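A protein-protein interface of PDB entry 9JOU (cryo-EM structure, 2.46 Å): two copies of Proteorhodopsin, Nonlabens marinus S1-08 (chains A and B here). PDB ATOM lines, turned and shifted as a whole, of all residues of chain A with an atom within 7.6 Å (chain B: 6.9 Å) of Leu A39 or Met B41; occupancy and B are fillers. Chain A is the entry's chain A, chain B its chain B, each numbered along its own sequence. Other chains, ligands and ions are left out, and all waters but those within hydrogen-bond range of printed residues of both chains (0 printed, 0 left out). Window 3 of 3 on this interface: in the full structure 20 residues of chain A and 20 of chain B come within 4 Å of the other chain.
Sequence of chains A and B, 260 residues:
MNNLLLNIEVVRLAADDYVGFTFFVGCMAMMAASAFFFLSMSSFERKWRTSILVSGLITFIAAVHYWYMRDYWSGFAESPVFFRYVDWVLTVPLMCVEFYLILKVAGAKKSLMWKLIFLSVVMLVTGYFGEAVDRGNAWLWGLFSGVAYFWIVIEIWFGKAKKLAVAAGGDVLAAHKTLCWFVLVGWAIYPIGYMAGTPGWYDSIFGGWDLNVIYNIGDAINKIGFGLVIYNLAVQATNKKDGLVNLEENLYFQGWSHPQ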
ATOM      1  N   ALA A  32     -20.202 -37.592  19.992  1.00  0.00           N
ATOM      2  CA  ALA A  32     -20.589 -36.519  20.900  1.00  0.00           C
ATOM      3  C   ALA A  32     -20.442 -35.157  20.244  1.00  0.00           C
ATOM      4  O   ALA A  32     -21.410 -34.390  20.176  1.00  0.00           O
ATOM      5  CB  ALA A  32     -19.743 -36.595  22.158  1.00  0.00           C
ATOM      6  N   ALA A  33     -19.227 -34.887  19.723  1.00  0.00           N
ATOM      7  CA  ALA A  33     -18.969 -33.678  18.944  1.00  0.00           C
ATOM      8  C   ALA A  33     -20.042 -33.511  17.840  1.00  0.00           C
ATOM      9  O   ALA A  33     -20.687 -32.464  17.733  1.00  0.00           O
ATOM     10  CB  ALA A  33     -17.572 -33.765  18.387  1.00  0.00           C
ATOM     11  N   SER A  34     -20.322 -34.549  17.056  1.00  0.00           N
ATOM     12  CA  SER A  34     -21.285 -34.373  15.961  1.00  0.00           C
ATOM     13  C   SER A  34     -22.615 -33.860  16.478  1.00  0.00           C
ATOM     14  O   SER A  34     -23.204 -32.943  15.893  1.00  0.00           O
ATOM     15  CB  SER A  34     -21.527 -35.613  15.163  1.00  0.00           C
ATOM     16  OG  SER A  34     -21.256 -36.786  15.926  1.00  0.00           O
ATOM     17  N   ALA A  35     -23.054 -34.450  17.607  1.00  0.00           N
ATOM     18  CA  ALA A  35     -24.285 -34.037  18.268  1.00  0.00           C
ATOM     19  C   ALA A  35     -24.156 -32.587  18.731  1.00  0.00           C
ATOM     20  O   ALA A  35     -25.111 -31.813  18.593  1.00  0.00           O
ATOM     21  CB  ALA A  35     -24.561 -34.949  19.408  1.00  0.00           C
ATOM     22  N   PHE A  36     -22.954 -32.242  19.232  1.00  0.00           N
ATOM     23  CA  PHE A  36     -22.741 -30.962  19.885  1.00  0.00           C
ATOM     24  C   PHE A  36     -22.841 -29.824  18.879  1.00  0.00           C
ATOM     25  O   PHE A  36     -23.426 -28.797  19.204  1.00  0.00           O
ATOM     26  CB  PHE A  36     -21.408 -30.926  20.656  1.00  0.00           C
ATOM     27  CG  PHE A  36     -20.953 -29.557  21.152  1.00  0.00           C
ATOM     28  CD1 PHE A  36     -21.569 -28.956  22.241  1.00  0.00           C
ATOM     29  CD2 PHE A  36     -19.913 -28.868  20.531  1.00  0.00           C
ATOM     30  CE1 PHE A  36     -21.150 -27.708  22.703  1.00  0.00           C
ATOM     31  CE2 PHE A  36     -19.525 -27.607  20.973  1.00  0.00           C
ATOM     32  CZ  PHE A  36     -20.142 -27.031  22.061  1.00  0.00           C
ATOM     33  N   PHE A  37     -22.304 -30.007  17.661  1.00  0.00           N
ATOM     34  CA  PHE A  37     -22.409 -28.990  16.611  1.00  0.00           C
ATOM     35  C   PHE A  37     -23.820 -28.986  16.004  1.00  0.00           C
ATOM     36  O   PHE A  37     -24.420 -27.932  15.807  1.00  0.00           O
ATOM     37  CB  PHE A  37     -21.349 -29.227  15.530  1.00  0.00           C
ATOM     38  CG  PHE A  37     -19.920 -29.209  16.051  1.00  0.00           C
ATOM     39  CD1 PHE A  37     -19.465 -28.189  16.853  1.00  0.00           C
ATOM     40  CD2 PHE A  37     -19.043 -30.247  15.767  1.00  0.00           C
ATOM     41  CE1 PHE A  37     -18.156 -28.177  17.311  1.00  0.00           C
ATOM     42  CE2 PHE A  37     -17.736 -30.233  16.220  1.00  0.00           C
ATOM     43  CZ  PHE A  37     -17.305 -29.209  17.017  1.00  0.00           C
ATOM     44  N   PHE A  38     -24.372 -30.154  15.696  1.00  0.00           N
ATOM     45  CA  PHE A  38     -25.731 -30.179  15.167  1.00  0.00           C
ATOM     46  C   PHE A  38     -26.715 -29.506  16.113  1.00  0.00           C
ATOM     47  O   PHE A  38     -27.627 -28.818  15.662  1.00  0.00           O
ATOM     48  CB  PHE A  38     -26.139 -31.636  14.947  1.00  0.00           C
ATOM     49  CG  PHE A  38     -25.414 -32.331  13.803  1.00  0.00           C
ATOM     50  CD1 PHE A  38     -24.952 -31.596  12.716  1.00  0.00           C
ATOM     51  CD2 PHE A  38     -25.240 -33.711  13.794  1.00  0.00           C
ATOM     52  CE1 PHE A  38     -24.318 -32.235  11.665  1.00  0.00           C
ATOM     53  CE2 PHE A  38     -24.589 -34.348  12.737  1.00  0.00           C
ATOM     54  CZ  PHE A  38     -24.139 -33.607  11.676  1.00  0.00           C
ATOM     55  N   LEU A  39     -26.556 -29.703  17.431  1.00  0.00           N
ATOM     56  CA  LEU A  39     -27.551 -29.199  18.372  1.00  0.00           C
ATOM     57  C   LEU A  39     -27.236 -27.760  18.766  1.00  0.00           C
ATOM     58  O   LEU A  39     -28.119 -27.072  19.277  1.00  0.00           O
ATOM     59  CB  LEU A  39     -27.657 -30.111  19.587  1.00  0.00           C
ATOM     60  CG  LEU A  39     -28.498 -31.375  19.376  1.00  0.00           C
ATOM     61  CD1 LEU A  39     -27.929 -32.549  20.164  1.00  0.00           C
ATOM     62  CD2 LEU A  39     -29.955 -31.142  19.710  1.00  0.00           C
ATOM     63  N   SER A  40     -26.001 -27.297  18.511  1.00  0.00           N
ATOM     64  CA  SER A  40     -25.672 -25.920  18.832  1.00  0.00           C
ATOM     65  C   SER A  40     -25.998 -25.010  17.660  1.00  0.00           C
ATOM     66  O   SER A  40     -26.114 -23.795  17.823  1.00  0.00           O
ATOM     67  CB  SER A  40     -24.240 -25.779  19.231  1.00  0.00           C
ATOM     68  OG  SER A  40     -23.765 -24.468  18.970  1.00  0.00           O
ATOM     69  N   MET A  41     -26.114 -25.610  16.472  1.00  0.00           N
ATOM     70  CA  MET A  41     -26.219 -24.872  15.224  1.00  0.00           C
ATOM     71  C   MET A  41     -27.255 -23.760  15.364  1.00  0.00           C
ATOM     72  O   MET A  41     -27.010 -22.646  14.917  1.00  0.00           O
ATOM     73  CB  MET A  41     -26.614 -25.832  14.104  1.00  0.00           C
ATOM     74  CG  MET A  41     -26.308 -25.350  12.714  1.00  0.00           C
ATOM     75  SD  MET A  41     -26.926 -26.589  11.563  1.00  0.00           S
ATOM     76  CE  MET A  41     -28.667 -26.220  11.817  1.00  0.00           C
ATOM     77  N   SER A  42     -28.381 -24.065  16.026  1.00  0.00           N
ATOM     78  CA  SER A  42     -29.544 -23.189  16.050  1.00  0.00           C
ATOM     79  C   SER A  42     -29.366 -21.996  16.988  1.00  0.00           C
ATOM     80  O   SER A  42     -30.183 -21.079  16.966  1.00  0.00           O
ATOM     81  CB  SER A  42     -30.789 -23.961  16.423  1.00  0.00           C
ATOM     82  OG  SER A  42     -31.922 -23.103  16.463  1.00  0.00           O
ATOM     83  N   SER A  43     -28.309 -21.986  17.807  1.00  0.00           N
ATOM     84  CA  SER A  43     -28.090 -20.913  18.768  1.00  0.00           C
ATOM     85  C   SER A  43     -27.202 -19.806  18.189  1.00  0.00           C
ATOM     86  O   SER A  43     -26.551 -19.067  18.926  1.00  0.00           O
ATOM     87  CB  SER A  43     -27.522 -21.466  20.063  1.00  0.00           C
ATOM     88  OG  SER A  43     -26.139 -21.768  19.942  1.00  0.00           O
ATOM     89  N   ILE A  52     -20.774 -24.124  11.035  1.00  0.00           N
ATOM     90  CA  ILE A  52     -20.859 -25.085  12.109  1.00  0.00           C
ATOM     91  C   ILE A  52     -21.343 -26.391  11.474  1.00  0.00           C
ATOM     92  O   ILE A  52     -20.633 -27.422  11.516  1.00  0.00           O
ATOM     93  CB  ILE A  52     -21.786 -24.585  13.242  1.00  0.00           C
ATOM     94  CG1 ILE A  52     -21.425 -23.229  13.792  1.00  0.00           C
ATOM     95  CG2 ILE A  52     -21.891 -25.618  14.352  1.00  0.00           C
ATOM     96  CD1 ILE A  52     -19.980 -23.112  14.166  1.00  0.00           C
ATOM     97  N   SER B  34     -31.074 -38.126  28.230  1.00  0.00           N
ATOM     98  CA  SER B  34     -30.441 -37.489  27.065  1.00  0.00           C
ATOM     99  C   SER B  34     -31.459 -36.813  26.172  1.00  0.00           C
ATOM    100  O   SER B  34     -31.261 -35.670  25.758  1.00  0.00           O
ATOM    101  CB  SER B  34     -29.608 -38.416  26.257  1.00  0.00           C
ATOM    102  OG  SER B  34     -30.059 -39.755  26.384  1.00  0.00           O
ATOM    103  N   ALA B  35     -32.588 -37.520  25.956  1.00  0.00           N
ATOM    104  CA  ALA B  35     -33.709 -36.996  25.183  1.00  0.00           C
ATOM    105  C   ALA B  35     -34.284 -35.774  25.864  1.00  0.00           C
ATOM    106  O   ALA B  35     -34.628 -34.792  25.194  1.00  0.00           O
ATOM    107  CB  ALA B  35     -34.730 -38.054  25.016  1.00  0.00           C
ATOM    108  N   PHE B  36     -34.339 -35.836  27.209  1.00  0.00           N
ATOM    109  CA  PHE B  36     -35.057 -34.838  27.991  1.00  0.00           C
ATOM    110  C   PHE B  36     -34.343 -33.501  27.914  1.00  0.00           C
ATOM    111  O   PHE B  36     -34.984 -32.470  27.781  1.00  0.00           O
ATOM    112  CB  PHE B  36     -35.316 -35.274  29.440  1.00  0.00           C
ATOM    113  CG  PHE B  36     -35.876 -34.175  30.346  1.00  0.00           C
ATOM    114  CD1 PHE B  36     -37.191 -33.729  30.227  1.00  0.00           C
ATOM    115  CD2 PHE B  36     -35.074 -33.580  31.322  1.00  0.00           C
ATOM    116  CE1 PHE B  36     -37.666 -32.690  31.023  1.00  0.00           C
ATOM    117  CE2 PHE B  36     -35.547 -32.539  32.102  1.00  0.00           C
ATOM    118  CZ  PHE B  36     -36.862 -32.119  31.980  1.00  0.00           C
ATOM    119  N   PHE B  37     -33.007 -33.517  27.975  1.00  0.00           N
ATOM    120  CA  PHE B  37     -32.217 -32.291  27.870  1.00  0.00           C
ATOM    121  C   PHE B  37     -32.140 -31.827  26.409  1.00  0.00           C
ATOM    122  O   PHE B  37     -32.280 -30.645  26.119  1.00  0.00           O
ATOM    123  CB  PHE B  37     -30.828 -32.521  28.461  1.00  0.00           C
ATOM    124  CG  PHE B  37     -30.840 -32.943  29.922  1.00  0.00           C
ATOM    125  CD1 PHE B  37     -31.589 -32.237  30.858  1.00  0.00           C
ATOM    126  CD2 PHE B  37     -30.132 -34.061  30.355  1.00  0.00           C
ATOM    127  CE1 PHE B  37     -31.587 -32.606  32.190  1.00  0.00           C
ATOM    128  CE2 PHE B  37     -30.145 -34.428  31.695  1.00  0.00           C
ATOM    129  CZ  PHE B  37     -30.871 -33.700  32.609  1.00  0.00           C
ATOM    130  N   PHE B  38     -31.920 -32.737  25.462  1.00  0.00           N
ATOM    131  CA  PHE B  38     -31.930 -32.331  24.065  1.00  0.00           C
ATOM    132  C   PHE B  38     -33.239 -31.641  23.687  1.00  0.00           C
ATOM    133  O   PHE B  38     -33.230 -30.666  22.948  1.00  0.00           O
ATOM    134  CB  PHE B  38     -31.684 -33.562  23.190  1.00  0.00           C
ATOM    135  CG  PHE B  38     -30.257 -34.095  23.280  1.00  0.00           C
ATOM    136  CD1 PHE B  38     -29.196 -33.250  23.612  1.00  0.00           C
ATOM    137  CD2 PHE B  38     -29.977 -35.434  23.019  1.00  0.00           C
ATOM    138  CE1 PHE B  38     -27.916 -33.758  23.729  1.00  0.00           C
ATOM    139  CE2 PHE B  38     -28.670 -35.920  23.123  1.00  0.00           C
ATOM    140  CZ  PHE B  38     -27.647 -35.079  23.497  1.00  0.00           C
ATOM    141  N   LEU B  39     -34.376 -32.160  24.167  1.00  0.00           N
ATOM    142  CA  LEU B  39     -35.669 -31.634  23.753  1.00  0.00           C
ATOM    143  C   LEU B  39     -36.059 -30.412  24.590  1.00  0.00           C
ATOM    144  O   LEU B  39     -36.945 -29.660  24.198  1.00  0.00           O
ATOM    145  CB  LEU B  39     -36.708 -32.740  23.869  1.00  0.00           C
ATOM    146  CG  LEU B  39     -36.986 -33.612  22.639  1.00  0.00           C
ATOM    147  CD1 LEU B  39     -37.649 -32.739  21.585  1.00  0.00           C
ATOM    148  CD2 LEU B  39     -35.820 -34.337  22.040  1.00  0.00           C
ATOM    149  N   SER B  40     -35.425 -30.234  25.761  1.00  0.00           N
ATOM    150  CA  SER B  40     -35.759 -29.104  26.605  1.00  0.00           C
ATOM    151  C   SER B  40     -34.886 -27.919  26.254  1.00  0.00           C
ATOM    152  O   SER B  40     -35.201 -26.799  26.618  1.00  0.00           O
ATOM    153  CB  SER B  40     -35.634 -29.439  28.058  1.00  0.00           C
ATOM    154  OG  SER B  40     -36.255 -30.687  28.318  1.00  0.00           O
ATOM    155  N   MET B  41     -33.776 -28.184  25.559  1.00  0.00           N
ATOM    156  CA  MET B  41     -32.765 -27.182  25.259  1.00  0.00           C
ATOM    157  C   MET B  41     -33.440 -25.915  24.741  1.00  0.00           C
ATOM    158  O   MET B  41     -33.079 -24.817  25.155  1.00  0.00           O
ATOM    159  CB  MET B  41     -31.792 -27.735  24.222  1.00  0.00           C
ATOM    160  CG  MET B  41     -30.460 -27.025  24.169  1.00  0.00           C
ATOM    161  SD  MET B  41     -29.417 -27.821  22.938  1.00  0.00           S
ATOM    162  CE  MET B  41     -29.455 -29.580  23.319  1.00  0.00           C
ATOM    163  N   SER B  42     -34.465 -26.085  23.891  1.00  0.00           N
ATOM    164  CA  SER B  42     -35.138 -24.988  23.206  1.00  0.00           C
ATOM    165  C   SER B  42     -36.033 -24.162  24.133  1.00  0.00           C
ATOM    166  O   SER B  42     -36.484 -23.099  23.738  1.00  0.00           O
ATOM    167  CB  SER B  42     -35.949 -25.520  22.046  1.00  0.00           C
ATOM    168  OG  SER B  42     -36.673 -24.484  21.393  1.00  0.00           O
ATOM    169  N   SER B  43     -36.278 -24.632  25.361  1.00  0.00           N
ATOM    170  CA  SER B  43     -37.220 -24.008  26.272  1.00  0.00           C
ATOM    171  C   SER B  43     -36.558 -22.947  27.160  1.00  0.00           C
ATOM    172  O   SER B  43     -37.126 -22.580  28.189  1.00  0.00           O
ATOM    173  CB  SER B  43     -37.904 -25.081  27.093  1.00  0.00           C
ATOM    174  OG  SER B  43     -38.905 -25.752  26.338  1.00  0.00           O
ATOM    175  N   PHE B  44     -35.358 -22.475  26.789  1.00  0.00           N
ATOM    176  CA  PHE B  44     -34.599 -21.588  27.663  1.00  0.00           C
ATOM    177  C   PHE B  44     -34.018 -20.440  26.845  1.00  0.00           C
ATOM    178  O   PHE B  44     -33.965 -20.491  25.622  1.00  0.00           O
ATOM    179  CB  PHE B  44     -33.431 -22.236  28.408  1.00  0.00           C
ATOM    180  CG  PHE B  44     -33.790 -23.368  29.356  1.00  0.00           C
ATOM    181  CD1 PHE B  44     -34.525 -23.122  30.510  1.00  0.00           C
ATOM    182  CD2 PHE B  44     -33.369 -24.673  29.095  1.00  0.00           C
ATOM    183  CE1 PHE B  44     -34.877 -24.168  31.345  1.00  0.00           C
ATOM    184  CE2 PHE B  44     -33.696 -25.701  29.951  1.00  0.00           C
ATOM    185  CZ  PHE B  44     -34.439 -25.443  31.076  1.00  0.00           C
ATOM    186  N   GLU B  45     -33.610 -19.371  27.537  1.00  0.00           N
ATOM    187  CA  GLU B  45     -32.924 -18.248  26.913  1.00  0.00           C
ATOM    188  C   GLU B  45     -31.561 -18.733  26.433  1.00  0.00           C
ATOM    189  O   GLU B  45     -31.114 -19.775  26.865  1.00  0.00           O
ATOM    190  CB  GLU B  45     -32.897 -17.086  27.906  1.00  0.00           C
ATOM    191  CG  GLU B  45     -32.053 -15.875  27.516  1.00  0.00           C
ATOM    192  CD  GLU B  45     -30.595 -15.952  27.925  1.00  0.00           C
ATOM    193  OE1 GLU B  45     -30.364 -15.997  29.150  1.00  0.00           O
ATOM    194  OE2 GLU B  45     -29.696 -15.954  27.052  1.00  0.00           O
ATOM    195  N   TRP B  48     -28.314 -20.200  28.671  1.00  0.00           N
ATOM    196  CA  TRP B  48     -28.453 -21.463  29.373  1.00  0.00           C
ATOM    197  C   TRP B  48     -28.326 -22.649  28.427  1.00  0.00           C
ATOM    198  O   TRP B  48     -27.725 -23.647  28.812  1.00  0.00           O
ATOM    199  CB  TRP B  48     -29.772 -21.502  30.156  1.00  0.00           C
ATOM    200  CG  TRP B  48     -29.755 -20.554  31.324  1.00  0.00           C
ATOM    201  CD1 TRP B  48     -28.793 -20.463  32.285  1.00  0.00           C
ATOM    202  CD2 TRP B  48     -30.708 -19.512  31.617  1.00  0.00           C
ATOM    203  NE1 TRP B  48     -29.081 -19.452  33.160  1.00  0.00           N
ATOM    204  CE2 TRP B  48     -30.241 -18.842  32.771  1.00  0.00           C
ATOM    205  CE3 TRP B  48     -31.900 -19.084  31.023  1.00  0.00           C
ATOM    206  CZ2 TRP B  48     -30.939 -17.780  33.340  1.00  0.00           C
ATOM    207  CZ3 TRP B  48     -32.589 -18.036  31.592  1.00  0.00           C
ATOM    208  CH2 TRP B  48     -32.112 -17.391  32.732  1.00  0.00           C
ATOM    209  N   ARG B  49     -28.820 -22.537  27.192  1.00  0.00           N
ATOM    210  CA  ARG B  49     -28.841 -23.654  26.249  1.00  0.00           C
ATOM    211  C   ARG B  49     -27.562 -24.500  26.317  1.00  0.00           C
ATOM    212  O   ARG B  49     -27.619 -25.723  26.455  1.00  0.00           O
ATOM    213  CB  ARG B  49     -28.986 -23.176  24.807  1.00  0.00           C
ATOM    214  CG  ARG B  49     -30.375 -23.315  24.219  1.00  0.00           C
ATOM    215  CD  ARG B  49     -31.313 -22.330  24.809  1.00  0.00           C
ATOM    216  NE  ARG B  49     -32.551 -22.314  24.011  1.00  0.00           N
ATOM    217  CZ  ARG B  49     -32.715 -21.575  22.923  1.00  0.00           C
ATOM    218  NH1 ARG B  49     -31.654 -20.977  22.396  1.00  0.00           N
ATOM    219  NH2 ARG B  49     -33.910 -21.419  22.369  1.00  0.00           N
ATOM    220  N   THR B  50     -26.406 -23.846  26.212  1.00  0.00           N
ATOM    221  CA  THR B  50     -25.164 -24.590  26.101  1.00  0.00           C
ATOM    222  C   THR B  50     -25.004 -25.482  27.330  1.00  0.00           C
ATOM    223  O   THR B  50     -24.581 -26.626  27.208  1.00  0.00           O
ATOM    224  CB  THR B  50     -23.915 -23.734  25.864  1.00  0.00           C
ATOM    225  OG1 THR B  50     -23.264 -23.450  27.099  1.00  0.00           O
ATOM    226  CG2 THR B  50     -24.156 -22.470  25.050  1.00  0.00           C
ATOM    227  N   ILE B  52     -27.304 -26.821  29.217  1.00  0.00           N
ATOM    228  CA  ILE B  52     -28.178 -27.959  29.100  1.00  0.00           C
ATOM    229  C   ILE B  52     -27.517 -28.905  28.097  1.00  0.00           C
ATOM    230  O   ILE B  52     -27.160 -30.050  28.432  1.00  0.00           O
ATOM    231  CB  ILE B  52     -29.594 -27.499  28.678  1.00  0.00           C
ATOM    232  CG1 ILE B  52     -30.214 -26.438  29.586  1.00  0.00           C
ATOM    233  CG2 ILE B  52     -30.521 -28.664  28.452  1.00  0.00           C
ATOM    234  CD1 ILE B  52     -29.747 -26.464  31.015  1.00  0.00           C
ATOM    235  N   LEU B  53     -27.290 -28.404  26.867  1.00  0.00           N
ATOM    236  CA  LEU B  53     -26.783 -29.216  25.775  1.00  0.00           C
ATOM    237  C   LEU B  53     -25.727 -30.155  26.308  1.00  0.00           C
ATOM    238  O   LEU B  53     -25.893 -31.366  26.146  1.00  0.00           O
ATOM    239  CB  LEU B  53     -26.205 -28.279  24.707  1.00  0.00           C
ATOM    240  CG  LEU B  53     -25.358 -28.860  23.564  1.00  0.00           C
ATOM    241  CD1 LEU B  53     -26.164 -29.437  22.451  1.00  0.00           C
ATOM    242  CD2 LEU B  53     -24.445 -27.771  23.007  1.00  0.00           C
ATOM    243  N   VAL B  54     -24.669 -29.579  26.952  1.00  0.00           N
ATOM    244  CA  VAL B  54     -23.555 -30.358  27.453  1.00  0.00           C
ATOM    245  C   VAL B  54     -24.020 -31.406  28.457  1.00  0.00           C
ATOM    246  O   VAL B  54     -23.539 -32.545  28.395  1.00  0.00           O
ATOM    247  CB  VAL B  54     -22.399 -29.539  28.037  1.00  0.00           C
ATOM    248  CG1 VAL B  54     -21.762 -28.633  26.979  1.00  0.00           C
ATOM    249  CG2 VAL B  54     -22.852 -28.743  29.237  1.00  0.00           C
ATOM    250  N   GLY B  56     -26.923 -32.908  28.512  1.00  0.00           N
ATOM    251  CA  GLY B  56     -27.387 -33.948  27.617  1.00  0.00           C
ATOM    252  C   GLY B  56     -26.241 -34.766  27.011  1.00  0.00           C
ATOM    253  O   GLY B  56     -26.206 -35.998  27.194  1.00  0.00           O
ATOM    254  N   LEU B  57     -25.300 -34.106  26.304  1.00  0.00           N
ATOM    255  CA  LEU B  57     -24.161 -34.850  25.790  1.00  0.00           C
ATOM    256  C   LEU B  57     -23.631 -35.860  26.795  1.00  0.00           C
ATOM    257  O   LEU B  57     -23.469 -37.031  26.419  1.00  0.00           O
ATOM    258  CB  LEU B  57     -23.010 -33.978  25.288  1.00  0.00           C
ATOM    259  CG  LEU B  57     -23.194 -33.444  23.864  1.00  0.00           C
ATOM    260  CD1 LEU B  57     -23.672 -34.471  22.881  1.00  0.00           C
ATOM    261  CD2 LEU B  57     -24.197 -32.344  23.862  1.00  0.00           C
ATOM    262  N   PHE B  60     -25.852 -38.534  27.052  1.00  0.00           N
ATOM    263  CA  PHE B  60     -25.849 -39.241  25.769  1.00  0.00           C
ATOM    264  C   PHE B  60     -24.675 -40.207  25.641  1.00  0.00           C
ATOM    265  O   PHE B  60     -24.873 -41.373  25.330  1.00  0.00           O
ATOM    266  CB  PHE B  60     -25.905 -38.188  24.663  1.00  0.00           C
ATOM    267  CG  PHE B  60     -25.939 -38.788  23.274  1.00  0.00           C
ATOM    268  CD1 PHE B  60     -26.700 -39.912  23.003  1.00  0.00           C
ATOM    269  CD2 PHE B  60     -25.156 -38.252  22.256  1.00  0.00           C
ATOM    270  CE1 PHE B  60     -26.680 -40.486  21.746  1.00  0.00           C
ATOM    271  CE2 PHE B  60     -25.169 -38.811  20.986  1.00  0.00           C
ATOM    272  CZ  PHE B  60     -25.922 -39.936  20.742  1.00  0.00           C
ATOM    273  N   TYR B 231     -30.705 -28.097  34.982  1.00  0.00           N
ATOM    274  CA  TYR B 231     -32.068 -27.796  34.582  1.00  0.00           C
ATOM    275  C   TYR B 231     -32.856 -27.017  35.634  1.00  0.00           C
ATOM    276  O   TYR B 231     -33.640 -26.124  35.281  1.00  0.00           O
ATOM    277  CB  TYR B 231     -32.847 -29.070  34.366  1.00  0.00           C
ATOM    278  CG  TYR B 231     -34.230 -28.794  33.785  1.00  0.00           C
ATOM    279  CD1 TYR B 231     -34.418 -28.505  32.436  1.00  0.00           C
ATOM    280  CD2 TYR B 231     -35.346 -28.859  34.600  1.00  0.00           C
ATOM    281  CE1 TYR B 231     -35.684 -28.292  31.915  1.00  0.00           C
ATOM    282  CE2 TYR B 231     -36.614 -28.664  34.087  1.00  0.00           C
ATOM    283  CZ  TYR B 231     -36.793 -28.386  32.745  1.00  0.00           C
ATOM    284  OH  TYR B 231     -38.071 -28.204  32.284  1.00  0.00           O
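O of Met B41 lies within hydrogen-bond range of NE of Arg B49, 2.8 Å away.
Among the printed residues, merely in contact across the chains: Ala A32 with Leu B57, Ala A35 with Leu B57, Phe A36 with Leu B53, Leu A39 with Phe B38, Leu A39 with Met B41 and Leu A39 with Leu B53.
Of the printed residues of chain B, Ala A32 touches Leu B57.
Of the printed residues of chain B, Phe A36 touches Leu B53.
Of chain B, only Phe B38, Met B41 and Leu B53 come within 4 Å of Leu A39.
Ala B35 touches none of the printed residues of chain A.
Of the printed residues of chain A, Phe B38 touches Leu A39 (3.7 Å).
Met B41 touches just one residue of chain A: Leu A39 (3.96 Å).
Of the printed residues of chain A, Leu B53 touches Phe A36 and Leu A39.
The nearest residue of chain B that does not touch Leu A39 is Leu B57 (5.3 Å).
The nearest residue of chain A that does not touch Met B41 is Ser A40 (5.6 Å).
Hydrophobic or aromatic side chains of chain A that line the printed part of chain B: Ala A35, Phe A36 and Leu A39.
Of the 22 printed residues of chain B, 4 touch a printed residue of chain A.
Printed residues of chain B that touch a printed residue of chain A: Phe B38, Met B41, Leu B53 and Leu B57.
Hydrophobic or aromatic side chains of chain B that line the printed part of chain A: Phe B38, Met B41, Leu B53 and Leu B57.
Among the printed residues, no Asp or Glu carboxylate lies within 4 Å of a Lys or Arg side-chain nitrogen of the other chain.
Leu A39 touches Phe B38, but with the chains exchanged Phe A38 does not touch Leu B39 (11.4 Å).
Leu A39 touches Met B41, but with the chains exchanged Met A41 does not touch Leu B39 (13.1 Å).
Positions printed for both chains: 34, 35, 36, 37, 38, 39, 40, 41, 42, 43 and 52.
Of the 6 pairs that touch across the chains among the printed residues, none has its exchanged pair printed and touching as well.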
